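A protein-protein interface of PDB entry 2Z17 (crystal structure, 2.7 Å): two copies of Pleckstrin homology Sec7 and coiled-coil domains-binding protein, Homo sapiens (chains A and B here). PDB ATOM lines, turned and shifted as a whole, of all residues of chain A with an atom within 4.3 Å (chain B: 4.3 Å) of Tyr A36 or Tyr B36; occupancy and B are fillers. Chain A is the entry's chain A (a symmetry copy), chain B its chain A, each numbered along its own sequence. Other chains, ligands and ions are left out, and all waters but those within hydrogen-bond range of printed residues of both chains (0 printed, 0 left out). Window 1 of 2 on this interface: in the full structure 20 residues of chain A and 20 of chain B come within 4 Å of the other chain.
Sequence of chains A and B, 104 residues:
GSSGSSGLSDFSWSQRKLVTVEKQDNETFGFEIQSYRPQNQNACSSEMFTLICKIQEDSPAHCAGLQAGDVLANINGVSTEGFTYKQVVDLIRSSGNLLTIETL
Printed residues of chain B within 4 Å of Tyr A36: Tyr B36 (3.9 Å), Arg B37 (3.3 Å), Pro B38 (3.8 Å) and Phe B49 (3.2 Å).
Tyr B36 touches just these residues of chain A: Tyr A36, Arg A37, Pro A38 and Phe A49.
Of the printed residues of chain A, Gln B34 touches Pro A38 (3.5 Å).
Printed residues of chain A within 4 Å of Phe B49: Tyr A36 (3.2 Å).
Of the printed residues of chain B, Ser A35 touches Arg B37 and Pro B38.
Met A48 touches none of the printed residues of chain B.
The nearest printed residue of chain A that does not touch Tyr B36 is Ser A35 (6.9 Å).
Printed residues of chain B that touch a printed residue of chain A: Gln B34, Ser B35, Tyr B36, Arg B37, Pro B38 and Phe B49.
Hydrophobic or aromatic side chains of chain B within 4 Å of the printed part of chain A: Tyr B36, Pro B38 and Phe B49.
Printed residues of chain A that touch a printed residue of chain B: Gln A34, Ser A35, Tyr A36, Arg A37, Pro A38 and Phe A49.
Among the printed residues, no Asp or Glu carboxylate lies within 4 Å of a Lys or Arg side-chain nitrogen of the other chain.
Among the printed residues, merely in contact across the chains: Gln A34 with Pro B38 (3.5 Å), Ser A35 with Arg B37 (3.7 Å), Ser A35 with Pro B38 (3.4 Å), Tyr A36 with Tyr B36 (3.9 Å), Tyr A36 with Arg B37 (3.3 Å), Tyr A36 with Pro B38 (3.8 Å), Tyr A36 with Phe B49 (3.2 Å), Arg A37 with Ser B35 (3.7 Å), Arg A37 with Tyr B36 (3.3 Å), Pro A38 with Gln B34 (3.5 Å), Pro A38 with Ser B35 (3.4 Å), Pro A38 with Tyr B36 (3.8 Å) and Phe A49 with Tyr B36 (3.2 Å).
The backbone carbonyl oxygen (O) of Leu B51 lies within hydrogen-bond range of the backbone NH (N) of Gln B34 (2.9 Å).
The backbone carbonyl oxygen of Phe B49 is in hydrogen-bond range of the backbone NH of Tyr B36 (2.8 Å).
O of Leu A51 lies within hydrogen-bond range of N of Gln A34, 2.9 Å away.
N of Tyr A36 lies within hydrogen-bond range of O of Phe A49 (2.8 Å).
The backbone NH of Arg B37 is in hydrogen-bond range of the backbone carbonyl oxygen of Arg A37 (2.8 Å).
Ser A35 touches Arg B37, and with the chains exchanged Arg A37 touches Ser B35.
Tyr B36 touches its own counterpart, Tyr A36.
Tyr A36 touches Arg B37, and with the chains exchanged Arg A37 touches Tyr B36.
Tyr A36 touches Phe B49, and with the chains exchanged Phe A49 touches Tyr B36.
Positions printed for both chains: 34, 35, 36, 37, 38, 48, 49 and 51.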
ATOM      1  N   GLN A  34      27.320  35.419  12.529  1.00  0.00           N
ATOM      2  CA  GLN A  34      28.111  34.360  13.074  1.00  0.00           C
ATOM      3  C   GLN A  34      28.681  33.500  11.984  1.00  0.00           C
ATOM      4  O   GLN A  34      27.944  32.901  11.240  1.00  0.00           O
ATOM      5  CB  GLN A  34      27.168  33.542  13.954  1.00  0.00           C
ATOM      6  CG  GLN A  34      27.542  33.503  15.369  1.00  0.00           C
ATOM      7  CD  GLN A  34      28.878  32.885  15.511  1.00  0.00           C
ATOM      8  OE1 GLN A  34      29.594  33.119  16.488  1.00  0.00           O
ATOM      9  NE2 GLN A  34      29.244  32.077  14.520  1.00  0.00           N
ATOM     10  N   SER A  35      29.990  33.424  11.875  1.00  0.00           N
ATOM     11  CA  SER A  35      30.583  32.575  10.858  1.00  0.00           C
ATOM     12  C   SER A  35      30.683  31.144  11.362  1.00  0.00           C
ATOM     13  O   SER A  35      31.083  30.922  12.493  1.00  0.00           O
ATOM     14  CB  SER A  35      31.978  33.066  10.492  1.00  0.00           C
ATOM     15  OG  SER A  35      31.943  33.905   9.353  1.00  0.00           O
ATOM     16  N   TYR A  36      30.318  30.170  10.531  1.00  0.00           N
ATOM     17  CA  TYR A  36      30.399  28.780  10.968  1.00  0.00           C
ATOM     18  C   TYR A  36      31.187  27.949  10.029  1.00  0.00           C
ATOM     19  O   TYR A  36      30.886  27.928   8.854  1.00  0.00           O
ATOM     20  CB  TYR A  36      29.031  28.134  11.087  1.00  0.00           C
ATOM     21  CG  TYR A  36      28.217  28.731  12.174  1.00  0.00           C
ATOM     22  CD1 TYR A  36      27.468  29.888  11.943  1.00  0.00           C
ATOM     23  CD2 TYR A  36      28.243  28.193  13.457  1.00  0.00           C
ATOM     24  CE1 TYR A  36      26.782  30.497  12.948  1.00  0.00           C
ATOM     25  CE2 TYR A  36      27.550  28.800  14.488  1.00  0.00           C
ATOM     26  CZ  TYR A  36      26.820  29.962  14.230  1.00  0.00           C
ATOM     27  OH  TYR A  36      26.144  30.608  15.257  1.00  0.00           O
ATOM     28  N   ARG A  37      32.180  27.248  10.563  1.00  0.00           N
ATOM     29  CA  ARG A  37      33.017  26.375   9.763  1.00  0.00           C
ATOM     30  C   ARG A  37      32.644  24.914   9.956  1.00  0.00           C
ATOM     31  O   ARG A  37      32.395  24.455  11.074  1.00  0.00           O
ATOM     32  CB  ARG A  37      34.493  26.555  10.117  1.00  0.00           C
ATOM     33  CG  ARG A  37      35.231  27.527   9.220  1.00  0.00           C
ATOM     34  CD  ARG A  37      36.720  27.496   9.515  1.00  0.00           C
ATOM     35  NE  ARG A  37      37.518  27.837   8.345  1.00  0.00           N
ATOM     36  CZ  ARG A  37      37.424  27.227   7.160  1.00  0.00           C
ATOM     37  NH1 ARG A  37      36.556  26.238   6.966  1.00  0.00           N
ATOM     38  NH2 ARG A  37      38.222  27.590   6.161  1.00  0.00           N
ATOM     39  N   PRO A  38      32.573  24.170   8.850  1.00  0.00           N
ATOM     40  CA  PRO A  38      32.242  22.747   8.836  1.00  0.00           C
ATOM     41  C   PRO A  38      33.458  21.862   9.113  1.00  0.00           C
ATOM     42  O   PRO A  38      34.437  21.921   8.392  1.00  0.00           O
ATOM     43  CB  PRO A  38      31.703  22.542   7.417  1.00  0.00           C
ATOM     44  CG  PRO A  38      32.464  23.538   6.625  1.00  0.00           C
ATOM     45  CD  PRO A  38      32.402  24.752   7.507  1.00  0.00           C
ATOM     46  N   MET A  48      33.264  28.266   4.892  1.00  0.00           N
ATOM     47  CA  MET A  48      32.630  29.400   5.526  1.00  0.00           C
ATOM     48  C   MET A  48      31.201  29.726   5.130  1.00  0.00           C
ATOM     49  O   MET A  48      30.817  29.627   3.965  1.00  0.00           O
ATOM     50  CB  MET A  48      33.482  30.637   5.214  1.00  0.00           C
ATOM     51  CG  MET A  48      33.738  31.584   6.355  1.00  0.00           C
ATOM     52  SD  MET A  48      34.676  30.828   7.656  1.00  0.00           S
ATOM     53  CE  MET A  48      33.334  30.447   8.731  1.00  0.00           C
ATOM     54  N   PHE A  49      30.431  30.138   6.128  1.00  0.00           N
ATOM     55  CA  PHE A  49      29.081  30.616   5.922  1.00  0.00           C
ATOM     56  C   PHE A  49      28.638  31.362   7.169  1.00  0.00           C
ATOM     57  O   PHE A  49      28.882  30.931   8.289  1.00  0.00           O
ATOM     58  CB  PHE A  49      28.131  29.492   5.496  1.00  0.00           C
ATOM     59  CG  PHE A  49      27.465  28.751   6.612  1.00  0.00           C
ATOM     60  CD1 PHE A  49      28.191  27.954   7.479  1.00  0.00           C
ATOM     61  CD2 PHE A  49      26.077  28.730   6.694  1.00  0.00           C
ATOM     62  CE1 PHE A  49      27.531  27.132   8.409  1.00  0.00           C
ATOM     63  CE2 PHE A  49      25.423  27.914   7.614  1.00  0.00           C
ATOM     64  CZ  PHE A  49      26.147  27.111   8.471  1.00  0.00           C
ATOM     65  N   LEU A  51      25.661  33.425   9.421  1.00  0.00           N
ATOM     66  CA  LEU A  51      24.235  33.454   9.702  1.00  0.00           C
ATOM     67  C   LEU A  51      23.845  34.533  10.716  1.00  0.00           C
ATOM     68  O   LEU A  51      24.636  34.917  11.565  1.00  0.00           O
ATOM     69  CB  LEU A  51      23.796  32.077  10.216  1.00  0.00           C
ATOM     70  CG  LEU A  51      22.966  31.895  11.500  1.00  0.00           C
ATOM     71  CD1 LEU A  51      22.570  30.434  11.536  1.00  0.00           C
ATOM     72  CD2 LEU A  51      23.717  32.276  12.782  1.00  0.00           C
ATOM     73  N   GLN B  34      26.359  17.390   9.943  1.00  0.00           N
ATOM     74  CA  GLN B  34      27.440  18.303   9.728  1.00  0.00           C
ATOM     75  C   GLN B  34      27.729  19.095  10.970  1.00  0.00           C
ATOM     76  O   GLN B  34      26.882  19.818  11.434  1.00  0.00           O
ATOM     77  CB  GLN B  34      26.987  19.229   8.602  1.00  0.00           C
ATOM     78  CG  GLN B  34      27.821  19.174   7.400  1.00  0.00           C
ATOM     79  CD  GLN B  34      29.203  19.578   7.737  1.00  0.00           C
ATOM     80  OE1 GLN B  34      30.164  19.212   7.056  1.00  0.00           O
ATOM     81  NE2 GLN B  34      29.328  20.348   8.815  1.00  0.00           N
ATOM     82  N   SER B  35      28.918  18.975  11.519  1.00  0.00           N
ATOM     83  CA  SER B  35      29.251  19.751  12.700  1.00  0.00           C
ATOM     84  C   SER B  35      29.732  21.137  12.298  1.00  0.00           C
ATOM     85  O   SER B  35      30.520  21.266  11.376  1.00  0.00           O
ATOM     86  CB  SER B  35      30.347  19.064  13.504  1.00  0.00           C
ATOM     87  OG  SER B  35      29.800  18.271  14.541  1.00  0.00           O
ATOM     88  N   TYR B  36      29.259  22.176  12.981  1.00  0.00           N
ATOM     89  CA  TYR B  36      29.692  23.526  12.635  1.00  0.00           C
ATOM     90  C   TYR B  36      30.230  24.252  13.807  1.00  0.00           C
ATOM     91  O   TYR B  36      29.554  24.350  14.810  1.00  0.00           O
ATOM     92  CB  TYR B  36      28.561  24.368  12.075  1.00  0.00           C
ATOM     93  CG  TYR B  36      28.084  23.873  10.761  1.00  0.00           C
ATOM     94  CD1 TYR B  36      27.136  22.848  10.692  1.00  0.00           C
ATOM     95  CD2 TYR B  36      28.626  24.366   9.578  1.00  0.00           C
ATOM     96  CE1 TYR B  36      26.748  22.325   9.498  1.00  0.00           C
ATOM     97  CE2 TYR B  36      28.242  23.843   8.357  1.00  0.00           C
ATOM     98  CZ  TYR B  36      27.300  22.813   8.320  1.00  0.00           C
ATOM     99  OH  TYR B  36      26.924  22.250   7.108  1.00  0.00           O
ATOM    100  N   ARG B  37      31.440  24.780  13.661  1.00  0.00           N
ATOM    101  CA  ARG B  37      32.077  25.538  14.721  1.00  0.00           C
ATOM    102  C   ARG B  37      32.018  27.033  14.452  1.00  0.00           C
ATOM    103  O   ARG B  37      32.237  27.494  13.329  1.00  0.00           O
ATOM    104  CB  ARG B  37      33.540  25.127  14.885  1.00  0.00           C
ATOM    105  CG  ARG B  37      33.773  24.079  15.954  1.00  0.00           C
ATOM    106  CD  ARG B  37      35.260  23.875  16.183  1.00  0.00           C
ATOM    107  NE  ARG B  37      35.551  23.450  17.545  1.00  0.00           N
ATOM    108  CZ  ARG B  37      35.154  24.098  18.644  1.00  0.00           C
ATOM    109  NH1 ARG B  37      34.432  25.211  18.557  1.00  0.00           N
ATOM    110  NH2 ARG B  37      35.500  23.645  19.844  1.00  0.00           N
ATOM    111  N   PRO B  38      31.690  27.808  15.488  1.00  0.00           N
ATOM    112  CA  PRO B  38      31.592  29.265  15.427  1.00  0.00           C
ATOM    113  C   PRO B  38      32.949  29.948  15.603  1.00  0.00           C
ATOM    114  O   PRO B  38      33.604  29.760  16.612  1.00  0.00           O
ATOM    115  CB  PRO B  38      30.641  29.586  16.583  1.00  0.00           C
ATOM    116  CG  PRO B  38      30.927  28.509  17.559  1.00  0.00           C
ATOM    117  CD  PRO B  38      30.986  27.295  16.677  1.00  0.00           C
ATOM    118  N   MET B  48      30.365  23.761  19.334  1.00  0.00           N
ATOM    119  CA  MET B  48      29.820  22.720  18.492  1.00  0.00           C
ATOM    120  C   MET B  48      28.310  22.626  18.370  1.00  0.00           C
ATOM    121  O   MET B  48      27.572  22.812  19.338  1.00  0.00           O
ATOM    122  CB  MET B  48      30.318  21.377  19.042  1.00  0.00           C
ATOM    123  CG  MET B  48      30.799  20.372  18.031  1.00  0.00           C
ATOM    124  SD  MET B  48      32.227  20.943  17.147  1.00  0.00           S
ATOM    125  CE  MET B  48      31.403  21.494  15.691  1.00  0.00           C
ATOM    126  N   PHE B  49      27.871  22.308  17.159  1.00  0.00           N
ATOM    127  CA  PHE B  49      26.475  22.046  16.882  1.00  0.00           C
ATOM    128  C   PHE B  49      26.376  21.343  15.539  1.00  0.00           C
ATOM    129  O   PHE B  49      27.048  21.702  14.580  1.00  0.00           O
ATOM    130  CB  PHE B  49      25.620  23.311  16.989  1.00  0.00           C
ATOM    131  CG  PHE B  49      25.493  24.115  15.734  1.00  0.00           C
ATOM    132  CD1 PHE B  49      26.582  24.769  15.186  1.00  0.00           C
ATOM    133  CD2 PHE B  49      24.236  24.344  15.185  1.00  0.00           C
ATOM    134  CE1 PHE B  49      26.410  25.657  14.109  1.00  0.00           C
ATOM    135  CE2 PHE B  49      24.065  25.225  14.120  1.00  0.00           C
ATOM    136  CZ  PHE B  49      25.149  25.885  13.581  1.00  0.00           C
ATOM    137  N   LEU B  51      24.066  19.695  12.355  1.00  0.00           N
ATOM    138  CA  LEU B  51      22.833  19.874  11.605  1.00  0.00           C
ATOM    139  C   LEU B  51      22.653  18.840  10.490  1.00  0.00           C
ATOM    140  O   LEU B  51      23.616  18.318   9.951  1.00  0.00           O
ATOM    141  CB  LEU B  51      22.809  21.289  11.010  1.00  0.00           C
ATOM    142  CG  LEU B  51      22.501  21.560   9.525  1.00  0.00           C
ATOM    143  CD1 LEU B  51      22.368  23.063   9.396  1.00  0.00           C
ATOM    144  CD2 LEU B  51      23.577  21.034   8.565  1.00  0.00           C
